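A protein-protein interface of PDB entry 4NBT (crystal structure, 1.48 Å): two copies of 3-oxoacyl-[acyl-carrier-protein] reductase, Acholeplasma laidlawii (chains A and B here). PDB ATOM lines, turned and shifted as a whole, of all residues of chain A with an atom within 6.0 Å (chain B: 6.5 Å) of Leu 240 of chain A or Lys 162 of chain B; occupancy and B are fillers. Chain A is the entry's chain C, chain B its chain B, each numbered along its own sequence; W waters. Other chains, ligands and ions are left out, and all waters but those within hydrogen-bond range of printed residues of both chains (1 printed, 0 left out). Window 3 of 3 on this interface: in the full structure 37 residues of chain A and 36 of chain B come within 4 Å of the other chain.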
ATOM      1  N   VAL A 134      19.095   0.999  -7.276  1.00  0.00           N
ATOM      2  CA  VAL A 134      18.950  -0.452  -7.301  1.00  0.00           C
ATOM      3  C   VAL A 134      20.055  -1.084  -8.152  1.00  0.00           C
ATOM      4  O   VAL A 134      20.519  -2.182  -7.858  1.00  0.00           O
ATOM      5  CB  VAL A 134      17.521  -0.841  -7.813  1.00  0.00           C
ATOM      6  CG1 VAL A 134      17.307  -0.415  -9.282  1.00  0.00           C
ATOM      7  CG2 VAL A 134      17.264  -2.316  -7.632  1.00  0.00           C
ATOM      8  N   VAL A 135      20.500  -0.385  -9.180  1.00  0.00           N
ATOM      9  CA  VAL A 135      21.577  -0.877 -10.050  1.00  0.00           C
ATOM     10  C   VAL A 135      22.917  -0.962  -9.307  1.00  0.00           C
ATOM     11  O   VAL A 135      23.728  -1.861  -9.589  1.00  0.00           O
ATOM     12  CB  VAL A 135      21.718  -0.033 -11.331  1.00  0.00           C
ATOM     13  CG1 VAL A 135      22.895  -0.485 -12.180  1.00  0.00           C
ATOM     14  CG2 VAL A 135      20.431  -0.085 -12.153  1.00  0.00           C
ATOM     15  N   PHE A 138      22.467  -4.279  -7.038  1.00  0.00           N
ATOM     16  CA  PHE A 138      22.314  -5.551  -7.739  1.00  0.00           C
ATOM     17  C   PHE A 138      23.116  -5.710  -9.044  1.00  0.00           C
ATOM     18  O   PHE A 138      23.168  -6.811  -9.602  1.00  0.00           O
ATOM     19  CB  PHE A 138      20.835  -5.799  -8.090  1.00  0.00           C
ATOM     20  CG  PHE A 138      19.955  -6.089  -6.914  1.00  0.00           C
ATOM     21  CD1 PHE A 138      19.886  -7.358  -6.374  1.00  0.00           C
ATOM     22  CD2 PHE A 138      19.203  -5.086  -6.352  1.00  0.00           C
ATOM     23  CE1 PHE A 138      19.051  -7.615  -5.290  1.00  0.00           C
ATOM     24  CE2 PHE A 138      18.376  -5.344  -5.271  1.00  0.00           C
ATOM     25  CZ  PHE A 138      18.299  -6.605  -4.752  1.00  0.00           C
ATOM     26  N   GLY A 139      23.688  -4.625  -9.551  1.00  0.00           N
ATOM     27  CA  GLY A 139      24.275  -4.628 -10.885  1.00  0.00           C
ATOM     28  C   GLY A 139      23.201  -4.618 -11.954  1.00  0.00           C
ATOM     29  O   GLY A 139      22.036  -4.898 -11.668  1.00  0.00           O
ATOM     30  N   ASN A 140      23.557  -4.312 -13.195  1.00  0.00           N
ATOM     31  CA  ASN A 140      22.587  -4.402 -14.278  1.00  0.00           C
ATOM     32  C   ASN A 140      23.299  -4.473 -15.596  1.00  0.00           C
ATOM     33  O   ASN A 140      24.264  -3.755 -15.831  1.00  0.00           O
ATOM     34  CB  ASN A 140      21.607  -3.225 -14.259  1.00  0.00           C
ATOM     35  CG  ASN A 140      20.415  -3.448 -15.163  1.00  0.00           C
ATOM     36  OD1 ASN A 140      19.910  -4.557 -15.310  1.00  0.00           O
ATOM     37  ND2 ASN A 140      19.960  -2.377 -15.788  1.00  0.00           N
ATOM     38  N   ILE A 141      22.820  -5.370 -16.446  1.00  0.00           N
ATOM     39  CA  ILE A 141      23.339  -5.536 -17.795  1.00  0.00           C
ATOM     40  C   ILE A 141      23.335  -4.204 -18.555  1.00  0.00           C
ATOM     41  O   ILE A 141      22.366  -3.432 -18.523  1.00  0.00           O
ATOM     42  CB  ILE A 141      22.501  -6.601 -18.538  1.00  0.00           C
ATOM     43  CG1 ILE A 141      22.722  -7.969 -17.885  1.00  0.00           C
ATOM     44  CG2 ILE A 141      22.854  -6.667 -20.028  1.00  0.00           C
ATOM     45  CD1 ILE A 141      21.710  -9.003 -18.287  1.00  0.00           C
ATOM     46  N   TYR A 180      13.015   1.913 -10.067  1.00  0.00           N
ATOM     47  CA  TYR A 180      12.729   2.639 -11.286  1.00  0.00           C
ATOM     48  C   TYR A 180      11.572   3.600 -11.135  1.00  0.00           C
ATOM     49  O   TYR A 180      10.500   3.227 -10.692  1.00  0.00           O
ATOM     50  CB  TYR A 180      12.519   1.643 -12.437  1.00  0.00           C
ATOM     51  CG  TYR A 180      13.828   0.988 -12.839  1.00  0.00           C
ATOM     52  CD1 TYR A 180      14.285  -0.159 -12.186  1.00  0.00           C
ATOM     53  CD2 TYR A 180      14.641   1.553 -13.802  1.00  0.00           C
ATOM     54  CE1 TYR A 180      15.483  -0.747 -12.531  1.00  0.00           C
ATOM     55  CE2 TYR A 180      15.861   0.969 -14.142  1.00  0.00           C
ATOM     56  CZ  TYR A 180      16.264  -0.169 -13.493  1.00  0.00           C
ATOM     57  OH  TYR A 180      17.478  -0.745 -13.839  1.00  0.00           O
ATOM     58  N   PHE A 197      11.045  -4.602 -15.234  1.00  0.00           N
ATOM     59  CA  PHE A 197      11.422  -4.061 -13.937  1.00  0.00           C
ATOM     60  C   PHE A 197      10.205  -3.901 -13.018  1.00  0.00           C
ATOM     61  O   PHE A 197      10.247  -4.251 -11.831  1.00  0.00           O
ATOM     62  CB  PHE A 197      12.131  -2.720 -14.104  1.00  0.00           C
ATOM     63  CG  PHE A 197      13.434  -2.795 -14.883  1.00  0.00           C
ATOM     64  CD1 PHE A 197      14.147  -3.980 -14.997  1.00  0.00           C
ATOM     65  CD2 PHE A 197      13.931  -1.662 -15.511  1.00  0.00           C
ATOM     66  CE1 PHE A 197      15.334  -4.024 -15.711  1.00  0.00           C
ATOM     67  CE2 PHE A 197      15.106  -1.714 -16.231  1.00  0.00           C
ATOM     68  CZ  PHE A 197      15.804  -2.885 -16.328  1.00  0.00           C
ATOM     69  N   LEU A 200       9.255  -7.148 -11.479  1.00  0.00           N
ATOM     70  CA  LEU A 200      10.219  -7.639 -10.491  1.00  0.00           C
ATOM     71  C   LEU A 200      10.024  -7.034  -9.102  1.00  0.00           C
ATOM     72  O   LEU A 200      10.700  -7.424  -8.163  1.00  0.00           O
ATOM     73  CB  LEU A 200      11.641  -7.304 -10.931  1.00  0.00           C
ATOM     74  CG  LEU A 200      12.189  -8.076 -12.130  1.00  0.00           C
ATOM     75  CD1 LEU A 200      13.554  -7.537 -12.558  1.00  0.00           C
ATOM     76  CD2 LEU A 200      12.285  -9.545 -11.807  1.00  0.00           C
ATOM     77  N   MET A 238      11.905  -4.677  -5.106  1.00  0.00           N
ATOM     78  CA  MET A 238      12.567  -5.240  -6.259  1.00  0.00           C
ATOM     79  C   MET A 238      13.819  -6.063  -5.914  1.00  0.00           C
ATOM     80  O   MET A 238      14.574  -5.686  -5.048  1.00  0.00           O
ATOM     81  CB  MET A 238      13.034  -4.050  -7.101  1.00  0.00           C
ATOM     82  CG  MET A 238      13.411  -4.379  -8.448  1.00  0.00           C
ATOM     83  SD  MET A 238      13.711  -2.865  -9.371  1.00  0.00           S
ATOM     84  CE  MET A 238      13.712  -3.672 -10.915  1.00  0.00           C
ATOM     85  N   ARG A 239      14.020  -7.160  -6.642  1.00  0.00           N
ATOM     86  CA  ARG A 239      15.327  -7.787  -6.774  1.00  0.00           C
ATOM     87  C   ARG A 239      15.617  -7.715  -8.272  1.00  0.00           C
ATOM     88  O   ARG A 239      14.792  -8.144  -9.087  1.00  0.00           O
ATOM     89  CB  ARG A 239      15.318  -9.237  -6.268  1.00  0.00           C
ATOM     90  CG  ARG A 239      15.144  -9.381  -4.757  1.00  0.00           C
ATOM     91  CD  ARG A 239      13.680  -9.286  -4.306  1.00  0.00           C
ATOM     92  NE  ARG A 239      12.881 -10.371  -4.866  1.00  0.00           N
ATOM     93  CZ  ARG A 239      11.646 -10.262  -5.341  1.00  0.00           C
ATOM     94  NH1 ARG A 239      10.987  -9.101  -5.310  1.00  0.00           N
ATOM     95  NH2 ARG A 239      11.042 -11.330  -5.839  1.00  0.00           N
ATOM     96  N   LEU A 240      16.721  -7.079  -8.652  1.00  0.00           N
ATOM     97  CA  LEU A 240      17.053  -6.893 -10.057  1.00  0.00           C
ATOM     98  C   LEU A 240      18.088  -7.910 -10.544  1.00  0.00           C
ATOM     99  O   LEU A 240      19.115  -8.113  -9.860  1.00  0.00           O
ATOM    100  CB  LEU A 240      17.596  -5.487 -10.240  1.00  0.00           C
ATOM    101  CG  LEU A 240      18.075  -5.097 -11.635  1.00  0.00           C
ATOM    102  CD1 LEU A 240      16.956  -5.189 -12.646  1.00  0.00           C
ATOM    103  CD2 LEU A 240      18.644  -3.708 -11.573  1.00  0.00           C
ATOM    104  OXT LEU A 240      17.887  -8.521 -11.603  1.00  0.00           O
ATOM    105  N   THR B 157      31.337  -6.185 -10.394  1.00  0.00           N
ATOM    106  CA  THR B 157      31.300  -7.636 -10.231  1.00  0.00           C
ATOM    107  C   THR B 157      29.918  -8.171 -10.535  1.00  0.00           C
ATOM    108  O   THR B 157      29.759  -9.113 -11.326  1.00  0.00           O
ATOM    109  CB  THR B 157      31.731  -8.018  -8.802  1.00  0.00           C
ATOM    110  OG1 THR B 157      33.098  -7.630  -8.620  1.00  0.00           O
ATOM    111  CG2 THR B 157      31.642  -9.511  -8.578  1.00  0.00           C
ATOM    112  N   MET B 158      28.901  -7.549  -9.944  1.00  0.00           N
ATOM    113  CA  MET B 158      27.548  -8.034 -10.139  1.00  0.00           C
ATOM    114  C   MET B 158      27.115  -7.827 -11.597  1.00  0.00           C
ATOM    115  O   MET B 158      26.479  -8.691 -12.211  1.00  0.00           O
ATOM    116  CB  MET B 158      26.588  -7.323  -9.185  1.00  0.00           C
ATOM    117  CG  MET B 158      26.820  -7.663  -7.731  1.00  0.00           C
ATOM    118  SD  MET B 158      25.640  -6.828  -6.637  1.00  0.00           S
ATOM    119  CE  MET B 158      26.179  -5.127  -6.794  1.00  0.00           C
ATOM    120  N   THR B 159      27.430  -6.659 -12.146  1.00  0.00           N
ATOM    121  CA  THR B 159      27.077  -6.358 -13.527  1.00  0.00           C
ATOM    122  C   THR B 159      27.684  -7.364 -14.498  1.00  0.00           C
ATOM    123  O   THR B 159      27.007  -7.892 -15.389  1.00  0.00           O
ATOM    124  CB  THR B 159      27.522  -4.925 -13.921  1.00  0.00           C
ATOM    125  OG1 THR B 159      26.750  -3.976 -13.165  1.00  0.00           O
ATOM    126  CG2 THR B 159      27.266  -4.694 -15.378  1.00  0.00           C
ATOM    127  N   TRP B 160      28.978  -7.628 -14.354  1.00  0.00           N
ATOM    128  CA  TRP B 160      29.656  -8.527 -15.282  1.00  0.00           C
ATOM    129  C   TRP B 160      29.306 -10.002 -15.088  1.00  0.00           C
ATOM    130  O   TRP B 160      29.301 -10.768 -16.053  1.00  0.00           O
ATOM    131  CB  TRP B 160      31.142  -8.319 -15.164  1.00  0.00           C
ATOM    132  CG  TRP B 160      31.628  -7.005 -15.733  1.00  0.00           C
ATOM    133  CD1 TRP B 160      31.057  -6.278 -16.752  1.00  0.00           C
ATOM    134  CD2 TRP B 160      32.806  -6.299 -15.350  1.00  0.00           C
ATOM    135  NE1 TRP B 160      31.813  -5.177 -17.019  1.00  0.00           N
ATOM    136  CE2 TRP B 160      32.887  -5.154 -16.167  1.00  0.00           C
ATOM    137  CE3 TRP B 160      33.794  -6.514 -14.382  1.00  0.00           C
ATOM    138  CZ2 TRP B 160      33.927  -4.251 -16.058  1.00  0.00           C
ATOM    139  CZ3 TRP B 160      34.826  -5.604 -14.268  1.00  0.00           C
ATOM    140  CH2 TRP B 160      34.877  -4.484 -15.100  1.00  0.00           C
ATOM    141  N   ALA B 161      28.991 -10.404 -13.852  1.00  0.00           N
ATOM    142  CA  ALA B 161      28.474 -11.748 -13.614  1.00  0.00           C
ATOM    143  C   ALA B 161      27.179 -11.968 -14.424  1.00  0.00           C
ATOM    144  O   ALA B 161      26.935 -13.039 -14.955  1.00  0.00           O
ATOM    145  CB  ALA B 161      28.262 -11.956 -12.131  1.00  0.00           C
ATOM    146  N   LYS B 162      26.377 -10.925 -14.574  1.00  0.00           N
ATOM    147  CA  LYS B 162      25.176 -11.031 -15.394  1.00  0.00           C
ATOM    148  C   LYS B 162      25.521 -10.975 -16.873  1.00  0.00           C
ATOM    149  O   LYS B 162      25.126 -11.841 -17.628  1.00  0.00           O
ATOM    150  CB  LYS B 162      24.198  -9.895 -15.058  1.00  0.00           C
ATOM    151  CG  LYS B 162      23.642  -9.932 -13.649  1.00  0.00           C
ATOM    152  CD  LYS B 162      22.868  -8.650 -13.289  1.00  0.00           C
ATOM    153  CE  LYS B 162      22.096  -8.824 -11.983  1.00  0.00           C
ATOM    154  NZ  LYS B 162      21.179  -7.667 -11.744  1.00  0.00           N
ATOM    155  N   GLU B 163      26.299  -9.984 -17.280  1.00  0.00           N
ATOM    156  CA  GLU B 163      26.544  -9.714 -18.702  1.00  0.00           C
ATOM    157  C   GLU B 163      27.323 -10.826 -19.399  1.00  0.00           C
ATOM    158  O   GLU B 163      26.965 -11.241 -20.512  1.00  0.00           O
ATOM    159  CB  GLU B 163      27.326  -8.414 -18.884  1.00  0.00           C
ATOM    160  CG  GLU B 163      26.535  -7.306 -19.441  1.00  0.00           C
ATOM    161  CD  GLU B 163      27.354  -6.053 -19.696  1.00  0.00           C
ATOM    162  OE1 GLU B 163      28.407  -6.098 -20.418  1.00  0.00           O
ATOM    163  OE2 GLU B 163      26.912  -5.039 -19.159  1.00  0.00           O
ATOM    164  N   PHE B 164      28.380 -11.322 -18.762  1.00  0.00           N
ATOM    165  CA  PHE B 164      29.294 -12.231 -19.448  1.00  0.00           C
ATOM    166  C   PHE B 164      28.778 -13.657 -19.450  1.00  0.00           C
ATOM    167  O   PHE B 164      29.356 -14.502 -20.138  1.00  0.00           O
ATOM    168  CB  PHE B 164      30.700 -12.177 -18.840  1.00  0.00           C
ATOM    169  CG  PHE B 164      31.386 -10.825 -18.967  1.00  0.00           C
ATOM    170  CD1 PHE B 164      31.135  -9.970 -20.033  1.00  0.00           C
ATOM    171  CD2 PHE B 164      32.269 -10.402 -18.001  1.00  0.00           C
ATOM    172  CE1 PHE B 164      31.791  -8.728 -20.130  1.00  0.00           C
ATOM    173  CE2 PHE B 164      32.917  -9.172 -18.085  1.00  0.00           C
ATOM    174  CZ  PHE B 164      32.668  -8.336 -19.150  1.00  0.00           C
ATOM    175  N   ALA B 165      27.693 -13.916 -18.709  1.00  0.00           N
ATOM    176  CA  ALA B 165      27.064 -15.233 -18.683  1.00  0.00           C
ATOM    177  C   ALA B 165      25.846 -15.295 -19.606  1.00  0.00           C
ATOM    178  O   ALA B 165      25.147 -16.305 -19.661  1.00  0.00           O
ATOM    179  CB  ALA B 165      26.679 -15.614 -17.253  1.00  0.00           C
ATOM    180  N   LEU B 166      25.578 -14.222 -20.337  1.00  0.00           N
ATOM    181  CA  LEU B 166      24.454 -14.237 -21.273  1.00  0.00           C
ATOM    182  C   LEU B 166      24.681 -15.280 -22.372  1.00  0.00           C
ATOM    183  O   LEU B 166      25.821 -15.638 -22.698  1.00  0.00           O
ATOM    184  CB  LEU B 166      24.241 -12.850 -21.877  1.00  0.00           C
ATOM    185  CG  LEU B 166      23.723 -11.748 -20.941  1.00  0.00           C
ATOM    186  CD1 LEU B 166      23.743 -10.400 -21.670  1.00  0.00           C
ATOM    187  CD2 LEU B 166      22.339 -12.082 -20.415  1.00  0.00           C
ATOM    188  N   VAL B 173      31.880 -14.325 -12.388  1.00  0.00           N
ATOM    189  CA  VAL B 173      32.547 -13.128 -11.912  1.00  0.00           C
ATOM    190  C   VAL B 173      32.253 -12.945 -10.446  1.00  0.00           C
ATOM    191  O   VAL B 173      31.083 -12.920 -10.053  1.00  0.00           O
ATOM    192  CB  VAL B 173      32.114 -11.876 -12.684  1.00  0.00           C
ATOM    193  CG1 VAL B 173      32.964 -10.685 -12.261  1.00  0.00           C
ATOM    194  CG2 VAL B 173      32.211 -12.106 -14.170  1.00  0.00           C
ATOM    195  N   THR B 228      28.695 -17.263  -8.406  1.00  0.00           N
ATOM    196  CA  THR B 228      28.915 -16.114  -9.265  1.00  0.00           C
ATOM    197  C   THR B 228      28.121 -14.915  -8.768  1.00  0.00           C
ATOM    198  O   THR B 228      27.082 -15.084  -8.100  1.00  0.00           O
ATOM    199  CB  THR B 228      28.595 -16.422 -10.741  1.00  0.00           C
ATOM    200  OG1 THR B 228      29.143 -15.372 -11.542  1.00  0.00           O
ATOM    201  CG2 THR B 228      27.099 -16.574 -10.986  1.00  0.00           C
ATOM    202  N   GLY B 229      28.613 -13.718  -9.072  1.00  0.00           N
ATOM    203  CA  GLY B 229      27.999 -12.482  -8.614  1.00  0.00           C
ATOM    204  C   GLY B 229      28.289 -12.116  -7.167  1.00  0.00           C
ATOM    205  O   GLY B 229      27.672 -11.182  -6.642  1.00  0.00           O
HETATM  206  O   HOH W   1      20.122  -7.050 -14.301  1.00  0.00           O
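NZ of Lys 162 of chain B lies within hydrogen-bond range of O of Phe 138 of chain A. NZ of Lys 162 of chain B is in salt-bridge range of O of Leu 240 of chain A (2.8 Å). The backbone carbonyl oxygen of Gly 139 of chain A lies within hydrogen-bond range of the side-chain amino group of Lys 162 of chain B, at 2.9 Å. OG1 of Thr 159 of chain B sits at hydrogen-bond distance from N of Asn 140 of chain A (3.2 Å).
Among the printed residues, merely in contact across the chains: Gly 139 of chain A with Thr 159 of chain B (3.4 Å), Phe 138 of chain A with Met 158 of chain B (3.5 Å), Ile 141 of chain A with Glu 163 of chain B (3.7 Å), Ile 141 of chain A with Lys 162 of chain B (3.7 Å), Gly 139 of chain A with Met 158 of chain B (3.7 Å) and Ile 141 of chain A with Leu 166 of chain B (3.8 Å).
Of the printed residues of chain B, Phe 138 of chain A touches Met 158 and Lys 162. Of the printed residues of chain B, Ile 141 of chain A touches Lys 162 (3.7 Å), Glu 163 (3.7 Å) and Leu 166 (3.8 Å). Leu 240 of chain A touches one residue of chain B. Of the printed residues of chain A, Thr 159 of chain B touches Gly 139 (3.4 Å) and Asn 140 (3.2 Å). Lys 162 of chain B touches just these residues of chain A: Phe 138, Gly 139, Ile 141 and Leu 240. Of the printed residues of chain A, Glu 163 of chain B touches Ile 141 (3.7 Å). Printed residues of chain A within 4 Å of Leu 166 of chain B: Ile 141. Val 173 of chain B touches none of the printed residues of chain A. The nearest printed residue of chain B that does not touch Leu 240 of chain A is Met 158 of chain B (7.4 Å). The nearest residue of chain A that does not touch Lys 162 of chain B is Asn 140 of chain A (4.4 Å). The nearest printed residue of chain A that does not touch Thr 159 of chain B is Ile 141 of chain A (4.6 Å).
Hydrophobic or aromatic side chains of chain B that line the printed part of chain A: Met 158 and Leu 166. Of the 12 printed residues of chain A, 5 touch a printed residue of chain B. Among the printed residues, no Asp or Glu carboxylate lies within 4 Å of a Lys or Arg side-chain nitrogen of the other chain.
No position is printed for both chains. Of the 10 pairs that touch across the chains among the printed residues, none has its exchanged pair printed and touching as well.
Water W1 lies within hydrogen-bond range of OD1 of Asn 140 of chain A and NZ of Lys 162 of chain B.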
